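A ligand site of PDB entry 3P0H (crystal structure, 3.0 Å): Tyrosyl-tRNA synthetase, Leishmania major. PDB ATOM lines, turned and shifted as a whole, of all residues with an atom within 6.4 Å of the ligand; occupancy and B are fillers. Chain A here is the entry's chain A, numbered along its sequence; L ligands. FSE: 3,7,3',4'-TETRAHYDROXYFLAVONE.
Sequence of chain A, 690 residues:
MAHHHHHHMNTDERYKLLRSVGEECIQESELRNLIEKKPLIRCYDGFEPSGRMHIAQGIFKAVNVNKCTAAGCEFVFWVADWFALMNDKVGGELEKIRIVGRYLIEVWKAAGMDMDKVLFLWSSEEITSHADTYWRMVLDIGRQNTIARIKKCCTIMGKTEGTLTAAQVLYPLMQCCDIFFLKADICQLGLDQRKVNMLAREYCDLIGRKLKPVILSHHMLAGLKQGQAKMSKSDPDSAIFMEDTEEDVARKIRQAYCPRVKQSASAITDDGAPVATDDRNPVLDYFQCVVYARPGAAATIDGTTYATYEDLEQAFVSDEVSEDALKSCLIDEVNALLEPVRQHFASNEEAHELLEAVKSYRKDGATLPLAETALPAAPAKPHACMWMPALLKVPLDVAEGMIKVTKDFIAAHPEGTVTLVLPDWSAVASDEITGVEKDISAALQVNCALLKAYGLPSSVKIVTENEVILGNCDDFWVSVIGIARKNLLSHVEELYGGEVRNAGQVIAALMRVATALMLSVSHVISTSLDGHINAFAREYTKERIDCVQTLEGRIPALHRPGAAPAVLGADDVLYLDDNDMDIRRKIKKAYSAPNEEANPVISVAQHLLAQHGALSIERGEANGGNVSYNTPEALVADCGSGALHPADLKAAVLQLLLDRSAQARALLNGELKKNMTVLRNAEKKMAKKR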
ATOM      1  N   TYR A  44      10.230 -14.178 -31.809  1.00  0.00           N
ATOM      2  CA  TYR A  44      11.303 -13.601 -31.013  1.00  0.00           C
ATOM      3  C   TYR A  44      12.246 -14.673 -30.493  1.00  0.00           C
ATOM      4  O   TYR A  44      11.837 -15.801 -30.197  1.00  0.00           O
ATOM      5  CB  TYR A  44      10.719 -12.758 -29.883  1.00  0.00           C
ATOM      6  CG  TYR A  44      11.334 -12.957 -28.529  1.00  0.00           C
ATOM      7  CD1 TYR A  44      12.425 -12.209 -28.118  1.00  0.00           C
ATOM      8  CD2 TYR A  44      10.800 -13.878 -27.641  1.00  0.00           C
ATOM      9  CE1 TYR A  44      12.989 -12.389 -26.862  1.00  0.00           C
ATOM     10  CE2 TYR A  44      11.343 -14.068 -26.391  1.00  0.00           C
ATOM     11  CZ  TYR A  44      12.430 -13.322 -25.998  1.00  0.00           C
ATOM     12  OH  TYR A  44      12.951 -13.527 -24.731  1.00  0.00           O
ATOM     13  N   ASP A  45      13.516 -14.314 -30.421  1.00  0.00           N
ATOM     14  CA  ASP A  45      14.547 -15.120 -29.789  1.00  0.00           C
ATOM     15  C   ASP A  45      15.568 -14.121 -29.245  1.00  0.00           C
ATOM     16  O   ASP A  45      15.472 -12.922 -29.534  1.00  0.00           O
ATOM     17  CB  ASP A  45      15.180 -16.094 -30.782  1.00  0.00           C
ATOM     18  CG  ASP A  45      15.856 -17.294 -30.114  1.00  0.00           C
ATOM     19  OD1 ASP A  45      16.058 -17.275 -28.879  1.00  0.00           O
ATOM     20  OD2 ASP A  45      16.203 -18.269 -30.806  1.00  0.00           O
ATOM     21  N   GLY A  46      16.502 -14.585 -28.441  1.00  0.00           N
ATOM     22  CA  GLY A  46      17.488 -13.694 -27.833  1.00  0.00           C
ATOM     23  C   GLY A  46      18.799 -14.399 -27.526  1.00  0.00           C
ATOM     24  O   GLY A  46      18.851 -15.633 -27.509  1.00  0.00           O
ATOM     25  N   PHE A  47      19.855 -13.612 -27.314  1.00  0.00           N
ATOM     26  CA  PHE A  47      21.157 -14.174 -26.988  1.00  0.00           C
ATOM     27  C   PHE A  47      22.123 -13.144 -26.413  1.00  0.00           C
ATOM     28  O   PHE A  47      22.004 -11.947 -26.703  1.00  0.00           O
ATOM     29  CB  PHE A  47      21.791 -14.824 -28.235  1.00  0.00           C
ATOM     30  CG  PHE A  47      21.964 -13.892 -29.394  1.00  0.00           C
ATOM     31  CD1 PHE A  47      23.166 -13.227 -29.602  1.00  0.00           C
ATOM     32  CD2 PHE A  47      20.942 -13.693 -30.311  1.00  0.00           C
ATOM     33  CE1 PHE A  47      23.335 -12.371 -30.683  1.00  0.00           C
ATOM     34  CE2 PHE A  47      21.101 -12.828 -31.390  1.00  0.00           C
ATOM     35  CZ  PHE A  47      22.310 -12.169 -31.570  1.00  0.00           C
ATOM     36  N   GLU A  48      23.039 -13.621 -25.574  1.00  0.00           N
ATOM     37  CA  GLU A  48      24.245 -12.868 -25.217  1.00  0.00           C
ATOM     38  C   GLU A  48      25.338 -13.290 -26.204  1.00  0.00           C
ATOM     39  O   GLU A  48      25.579 -14.486 -26.365  1.00  0.00           O
ATOM     40  CB  GLU A  48      24.729 -13.206 -23.794  1.00  0.00           C
ATOM     41  CG  GLU A  48      23.992 -12.518 -22.648  1.00  0.00           C
ATOM     42  CD  GLU A  48      24.424 -13.040 -21.270  1.00  0.00           C
ATOM     43  OE1 GLU A  48      25.408 -13.807 -21.187  1.00  0.00           O
ATOM     44  OE2 GLU A  48      23.755 -12.698 -20.261  1.00  0.00           O
ATOM     45  N   LYS A  61      19.627 -21.998 -36.617  1.00  0.00           N
ATOM     46  CA  LYS A  61      18.830 -20.804 -36.367  1.00  0.00           C
ATOM     47  C   LYS A  61      18.422 -20.140 -37.680  1.00  0.00           C
ATOM     48  O   LYS A  61      17.252 -19.768 -37.850  1.00  0.00           O
ATOM     49  CB  LYS A  61      19.574 -19.777 -35.510  1.00  0.00           C
ATOM     50  CG  LYS A  61      18.653 -18.704 -34.940  1.00  0.00           C
ATOM     51  CD  LYS A  61      17.777 -19.259 -33.827  1.00  0.00           C
ATOM     52  CE  LYS A  61      16.326 -18.877 -33.987  1.00  0.00           C
ATOM     53  NZ  LYS A  61      15.466 -19.607 -33.009  1.00  0.00           N
ATOM     54  N   TRP A  78      16.520 -10.355 -29.828  1.00  0.00           N
ATOM     55  CA  TRP A  78      16.797  -9.523 -28.658  1.00  0.00           C
ATOM     56  C   TRP A  78      18.243  -9.785 -28.258  1.00  0.00           C
ATOM     57  O   TRP A  78      18.561 -10.826 -27.680  1.00  0.00           O
ATOM     58  CB  TRP A  78      15.808  -9.857 -27.541  1.00  0.00           C
ATOM     59  CG  TRP A  78      15.981  -9.098 -26.266  1.00  0.00           C
ATOM     60  CD1 TRP A  78      16.470  -9.586 -25.091  1.00  0.00           C
ATOM     61  CD2 TRP A  78      15.646  -7.733 -26.019  1.00  0.00           C
ATOM     62  NE1 TRP A  78      16.478  -8.608 -24.134  1.00  0.00           N
ATOM     63  CE2 TRP A  78      15.972  -7.450 -24.679  1.00  0.00           C
ATOM     64  CE3 TRP A  78      15.098  -6.714 -26.803  1.00  0.00           C
ATOM     65  CZ2 TRP A  78      15.773  -6.200 -24.094  1.00  0.00           C
ATOM     66  CZ3 TRP A  78      14.907  -5.453 -26.233  1.00  0.00           C
ATOM     67  CH2 TRP A  78      15.247  -5.209 -24.887  1.00  0.00           C
ATOM     68  N   ALA A  80      21.175  -9.447 -26.061  1.00  0.00           N
ATOM     69  CA  ALA A  80      21.252  -9.193 -24.627  1.00  0.00           C
ATOM     70  C   ALA A  80      22.605  -8.602 -24.208  1.00  0.00           C
ATOM     71  O   ALA A  80      23.330  -9.197 -23.403  1.00  0.00           O
ATOM     72  CB  ALA A  80      20.975 -10.468 -23.854  1.00  0.00           C
ATOM     73  N   PHE A  83      24.011  -6.707 -20.357  1.00  0.00           N
ATOM     74  CA  PHE A  83      24.787  -7.439 -19.349  1.00  0.00           C
ATOM     75  C   PHE A  83      26.303  -7.194 -19.412  1.00  0.00           C
ATOM     76  O   PHE A  83      27.037  -7.585 -18.490  1.00  0.00           O
ATOM     77  CB  PHE A  83      24.504  -8.952 -19.446  1.00  0.00           C
ATOM     78  CG  PHE A  83      23.101  -9.333 -19.075  1.00  0.00           C
ATOM     79  CD1 PHE A  83      22.672  -9.241 -17.755  1.00  0.00           C
ATOM     80  CD2 PHE A  83      22.198  -9.792 -20.028  1.00  0.00           C
ATOM     81  CE1 PHE A  83      21.377  -9.588 -17.391  1.00  0.00           C
ATOM     82  CE2 PHE A  83      20.906 -10.155 -19.676  1.00  0.00           C
ATOM     83  CZ  PHE A  83      20.489 -10.051 -18.353  1.00  0.00           C
ATOM     84  N   MET A 174      13.562 -10.856 -15.910  1.00  0.00           N
ATOM     85  CA  MET A 174      13.903 -10.016 -17.054  1.00  0.00           C
ATOM     86  C   MET A 174      13.524 -10.691 -18.360  1.00  0.00           C
ATOM     87  O   MET A 174      12.834 -10.108 -19.195  1.00  0.00           O
ATOM     88  CB  MET A 174      15.398  -9.699 -17.048  1.00  0.00           C
ATOM     89  CG  MET A 174      15.843  -8.932 -15.828  1.00  0.00           C
ATOM     90  SD  MET A 174      17.744  -8.561 -15.862  1.00  0.00           S
ATOM     91  CE  MET A 174      17.993  -8.224 -13.961  1.00  0.00           C
ATOM     92  N   GLN A 175      13.975 -11.932 -18.529  1.00  0.00           N
ATOM     93  CA  GLN A 175      13.701 -12.692 -19.754  1.00  0.00           C
ATOM     94  C   GLN A 175      12.211 -12.741 -20.039  1.00  0.00           C
ATOM     95  O   GLN A 175      11.800 -12.578 -21.177  1.00  0.00           O
ATOM     96  CB  GLN A 175      14.263 -14.106 -19.670  1.00  0.00           C
ATOM     97  CG  GLN A 175      14.207 -14.872 -20.979  1.00  0.00           C
ATOM     98  CD  GLN A 175      14.922 -16.204 -20.910  1.00  0.00           C
ATOM     99  OE1 GLN A 175      15.899 -16.365 -20.171  1.00  0.00           O
ATOM    100  NE2 GLN A 175      14.452 -17.177 -21.692  1.00  0.00           N
ATOM    101  N   CYS A 176      11.419 -12.959 -18.996  1.00  0.00           N
ATOM    102  CA  CYS A 176       9.962 -13.011 -19.141  1.00  0.00           C
ATOM    103  C   CYS A 176       9.438 -11.664 -19.610  1.00  0.00           C
ATOM    104  O   CYS A 176       8.626 -11.592 -20.541  1.00  0.00           O
ATOM    105  CB  CYS A 176       9.293 -13.393 -17.818  1.00  0.00           C
ATOM    106  SG  CYS A 176       7.497 -13.529 -17.934  1.00  0.00           S
ATOM    107  N   ASP A 178      10.901  -9.431 -21.318  1.00  0.00           N
ATOM    108  CA  ASP A 178      11.301  -9.183 -22.704  1.00  0.00           C
ATOM    109  C   ASP A 178      10.184  -9.546 -23.670  1.00  0.00           C
ATOM    110  O   ASP A 178       9.917  -8.829 -24.626  1.00  0.00           O
ATOM    111  CB  ASP A 178      12.571  -9.952 -23.064  1.00  0.00           C
ATOM    112  CG  ASP A 178      13.781  -9.558 -22.214  1.00  0.00           C
ATOM    113  OD1 ASP A 178      13.780  -8.447 -21.645  1.00  0.00           O
ATOM    114  OD2 ASP A 178      14.739 -10.354 -22.112  1.00  0.00           O
ATOM    115  N   ILE A 179       9.516 -10.657 -23.388  1.00  0.00           N
ATOM    116  CA  ILE A 179       8.474 -11.192 -24.259  1.00  0.00           C
ATOM    117  C   ILE A 179       7.363 -10.167 -24.416  1.00  0.00           C
ATOM    118  O   ILE A 179       6.861  -9.973 -25.514  1.00  0.00           O
ATOM    119  CB  ILE A 179       7.897 -12.529 -23.721  1.00  0.00           C
ATOM    120  CG1 ILE A 179       8.958 -13.625 -23.743  1.00  0.00           C
ATOM    121  CG2 ILE A 179       6.702 -12.982 -24.551  1.00  0.00           C
ATOM    122  CD1 ILE A 179       8.554 -14.873 -23.023  1.00  0.00           C
ATOM    123  N   LEU A 182       8.784  -6.545 -25.991  1.00  0.00           N
ATOM    124  CA  LEU A 182       8.864  -6.566 -27.448  1.00  0.00           C
ATOM    125  C   LEU A 182       7.534  -6.891 -28.137  1.00  0.00           C
ATOM    126  O   LEU A 182       7.460  -6.856 -29.367  1.00  0.00           O
ATOM    127  CB  LEU A 182       9.890  -7.594 -27.895  1.00  0.00           C
ATOM    128  CG  LEU A 182      11.304  -7.401 -27.352  1.00  0.00           C
ATOM    129  CD1 LEU A 182      12.136  -8.644 -27.646  1.00  0.00           C
ATOM    130  CD2 LEU A 182      11.917  -6.140 -27.968  1.00  0.00           C
ATOM    131  N   GLN A 188       9.878 -18.066 -30.196  1.00  0.00           N
ATOM    132  CA  GLN A 188      10.633 -19.076 -30.938  1.00  0.00           C
ATOM    133  C   GLN A 188      12.050 -19.142 -30.367  1.00  0.00           C
ATOM    134  O   GLN A 188      12.983 -18.548 -30.881  1.00  0.00           O
ATOM    135  CB  GLN A 188      10.531 -18.796 -32.456  1.00  0.00           C
ATOM    136  CG  GLN A 188      11.642 -19.279 -33.383  1.00  0.00           C
ATOM    137  CD  GLN A 188      12.195 -20.647 -33.076  1.00  0.00           C
ATOM    138  OE1 GLN A 188      13.278 -20.990 -33.543  1.00  0.00           O
ATOM    139  NE2 GLN A 188      11.465 -21.431 -32.297  1.00  0.00           N
ATOM    140  N   LEU A 189      12.174 -19.866 -29.251  1.00  0.00           N
ATOM    141  CA  LEU A 189      13.461 -20.094 -28.575  1.00  0.00           C
ATOM    142  C   LEU A 189      13.707 -21.585 -28.485  1.00  0.00           C
ATOM    143  O   LEU A 189      12.866 -22.379 -28.894  1.00  0.00           O
ATOM    144  CB  LEU A 189      13.449 -19.517 -27.157  1.00  0.00           C
ATOM    145  CG  LEU A 189      13.338 -18.000 -27.052  1.00  0.00           C
ATOM    146  CD1 LEU A 189      11.886 -17.563 -27.241  1.00  0.00           C
ATOM    147  CD2 LEU A 189      13.889 -17.518 -25.722  1.00  0.00           C
ATOM    148  N   GLY A 190      14.851 -21.978 -27.960  1.00  0.00           N
ATOM    149  CA  GLY A 190      15.153 -23.384 -27.747  1.00  0.00           C
ATOM    150  C   GLY A 190      14.181 -24.016 -26.761  1.00  0.00           C
ATOM    151  O   GLY A 190      13.471 -23.343 -26.009  1.00  0.00           O
ATOM    152  N   LEU A 191      14.152 -25.353 -26.772  1.00  0.00           N
ATOM    153  CA  LEU A 191      13.330 -26.088 -25.830  1.00  0.00           C
ATOM    154  C   LEU A 191      13.916 -25.962 -24.428  1.00  0.00           C
ATOM    155  O   LEU A 191      13.188 -26.072 -23.461  1.00  0.00           O
ATOM    156  CB  LEU A 191      13.223 -27.559 -26.262  1.00  0.00           C
ATOM    157  CG  LEU A 191      12.077 -28.424 -25.717  1.00  0.00           C
ATOM    158  CD1 LEU A 191      10.725 -27.712 -25.767  1.00  0.00           C
ATOM    159  CD2 LEU A 191      12.024 -29.729 -26.517  1.00  0.00           C
ATOM    160  N   ASP A 192      15.218 -25.699 -24.313  1.00  0.00           N
ATOM    161  CA  ASP A 192      15.836 -25.539 -22.992  1.00  0.00           C
ATOM    162  C   ASP A 192      15.300 -24.339 -22.228  1.00  0.00           C
ATOM    163  O   ASP A 192      15.336 -24.330 -21.000  1.00  0.00           O
ATOM    164  CB  ASP A 192      17.363 -25.475 -23.087  1.00  0.00           C
ATOM    165  CG  ASP A 192      17.859 -24.331 -23.941  1.00  0.00           C
ATOM    166  OD1 ASP A 192      19.013 -23.906 -23.721  1.00  0.00           O
ATOM    167  OD2 ASP A 192      17.123 -23.870 -24.838  1.00  0.00           O
ATOM    168  N   GLN A 193      14.786 -23.333 -22.947  1.00  0.00           N
ATOM    169  CA  GLN A 193      14.208 -22.138 -22.334  1.00  0.00           C
ATOM    170  C   GLN A 193      12.694 -22.260 -22.165  1.00  0.00           C
ATOM    171  O   GLN A 193      11.983 -21.256 -22.064  1.00  0.00           O
ATOM    172  CB  GLN A 193      14.534 -20.897 -23.173  1.00  0.00           C
ATOM    173  CG  GLN A 193      16.024 -20.660 -23.395  1.00  0.00           C
ATOM    174  CD  GLN A 193      16.765 -20.385 -22.109  1.00  0.00           C
ATOM    175  OE1 GLN A 193      16.327 -19.564 -21.296  1.00  0.00           O
ATOM    176  NE2 GLN A 193      17.893 -21.053 -21.923  1.00  0.00           N
ATOM    177  N   HIS A 218      12.257 -24.852 -30.549  1.00  0.00           N
ATOM    178  CA  HIS A 218      13.036 -25.621 -31.524  1.00  0.00           C
ATOM    179  C   HIS A 218      13.901 -26.702 -30.863  1.00  0.00           C
ATOM    180  O   HIS A 218      14.166 -26.665 -29.661  1.00  0.00           O
ATOM    181  CB  HIS A 218      13.878 -24.703 -32.427  1.00  0.00           C
ATOM    182  CG  HIS A 218      14.941 -23.930 -31.712  1.00  0.00           C
ATOM    183  ND1 HIS A 218      16.117 -24.516 -31.271  1.00  0.00           N
ATOM    184  CD2 HIS A 218      15.037 -22.612 -31.400  1.00  0.00           C
ATOM    185  CE1 HIS A 218      16.866 -23.593 -30.694  1.00  0.00           C
ATOM    186  NE2 HIS A 218      16.235 -22.432 -30.759  1.00  0.00           N
ATOM    187  N   MET A 220      16.960 -29.078 -29.685  1.00  0.00           N
ATOM    188  CA  MET A 220      18.344 -28.934 -29.238  1.00  0.00           C
ATOM    189  C   MET A 220      19.191 -29.974 -29.949  1.00  0.00           C
ATOM    190  O   MET A 220      19.047 -31.174 -29.718  1.00  0.00           O
ATOM    191  CB  MET A 220      18.444 -29.121 -27.734  1.00  0.00           C
ATOM    192  CG  MET A 220      17.499 -28.250 -26.917  1.00  0.00           C
ATOM    193  SD  MET A 220      17.625 -26.327 -27.280  1.00  0.00           S
ATOM    194  CE  MET A 220      19.408 -25.948 -26.563  1.00  0.00           C
HETATM  195  C6  FSE L   1      17.228 -12.430 -22.944  1.00  0.00           C
HETATM  196  C5  FSE L   1      18.447 -13.107 -22.905  1.00  0.00           C
HETATM  197  C10 FSE L   1      18.534 -14.415 -23.392  1.00  0.00           C
HETATM  198  C9  FSE L   1      17.389 -14.999 -23.918  1.00  0.00           C
HETATM  199  C8  FSE L   1      16.171 -14.322 -23.957  1.00  0.00           C
HETATM  200  C7  FSE L   1      16.089 -13.029 -23.464  1.00  0.00           C
HETATM  201  C4  FSE L   1      19.742 -15.112 -23.360  1.00  0.00           C
HETATM  202  C3  FSE L   1      19.748 -16.400 -23.879  1.00  0.00           C
HETATM  203  C2  FSE L   1      18.605 -17.004 -24.392  1.00  0.00           C
HETATM  204  C1' FSE L   1      18.508 -18.282 -24.950  1.00  0.00           C
HETATM  205  C6' FSE L   1      19.180 -19.384 -24.431  1.00  0.00           C
HETATM  206  C5' FSE L   1      19.042 -20.650 -25.018  1.00  0.00           C
HETATM  207  C4' FSE L   1      18.218 -20.797 -26.133  1.00  0.00           C
HETATM  208  C3' FSE L   1      17.534 -19.708 -26.654  1.00  0.00           C
HETATM  209  C2' FSE L   1      17.682 -18.451 -26.069  1.00  0.00           C
HETATM  210  O1  FSE L   1      17.455 -16.279 -24.396  1.00  0.00           O
HETATM  211  O4  FSE L   1      20.757 -14.618 -22.895  1.00  0.00           O
HETATM  212  O3' FSE L   1      16.742 -19.916 -27.740  1.00  0.00           O
HETATM  213  O4' FSE L   1      18.047 -22.002 -26.747  1.00  0.00           O
HETATM  214  O3  FSE L   1      20.927 -17.073 -23.874  1.00  0.00           O
HETATM  215  O7  FSE L   1      14.904 -12.367 -23.509  1.00  0.00           O
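O of Gly 46 sits close to O1 of the ligand, 3.5 Å away. Merely in contact with the ligand: Glu 48 (3.7 Å), Trp 78 (3.6 Å), Ala 80 (3.8 Å), Gln 175 (3.6 Å), Leu 189 (3.4 Å), Gln 193 (3.3 Å) and His 218 (3.96 Å).
NE1 of Trp 78 lies within hydrogen-bond range of OD2 of Asp 178. N of Gly 190 is in hydrogen-bond range of NE2 of His 218 (3.2 Å). The backbone NH of Trp 78 is in hydrogen-bond range of the backbone carbonyl oxygen of Asp 45 (2.8 Å). The side-chain carboxylate (OD2) of Asp 45 lies within salt-bridge range of the side-chain amino group (NZ) of Lys 61 (2.7 Å). OE1 of Gln 193 lies within hydrogen-bond range of NE2 of Gln 175. The backbone NH (N) of His 218 lies within hydrogen-bond range of the backbone carbonyl oxygen (O) of Leu 189 (3.0 Å). The backbone NH (N) of Phe 47 sits at hydrogen-bond distance from the backbone carbonyl oxygen (O) of Trp 78 (3.1 Å). O of His 218 lies within hydrogen-bond range of N of Leu 191, at 3.2 Å.
An oxygen (O7) of the ligand lies within hydrogen-bond range of the side-chain carboxylate (OD2) of Asp 178 (2.5 Å). An oxygen (O7) of the ligand is in hydrogen-bond range of the side-chain hydroxyl (OH) of Tyr 44 (2.6 Å). The backbone NH (N) of Gly 190 is in hydrogen-bond range of an oxygen (O3') of the ligand (2.8 Å). O4' of the ligand is in hydrogen-bond range of OD2 of Asp 192, at 2.8 Å. The side-chain carboxylate of Asp 45 lies within hydrogen-bond range of an oxygen (O3') of the ligand, 3.0 Å away.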
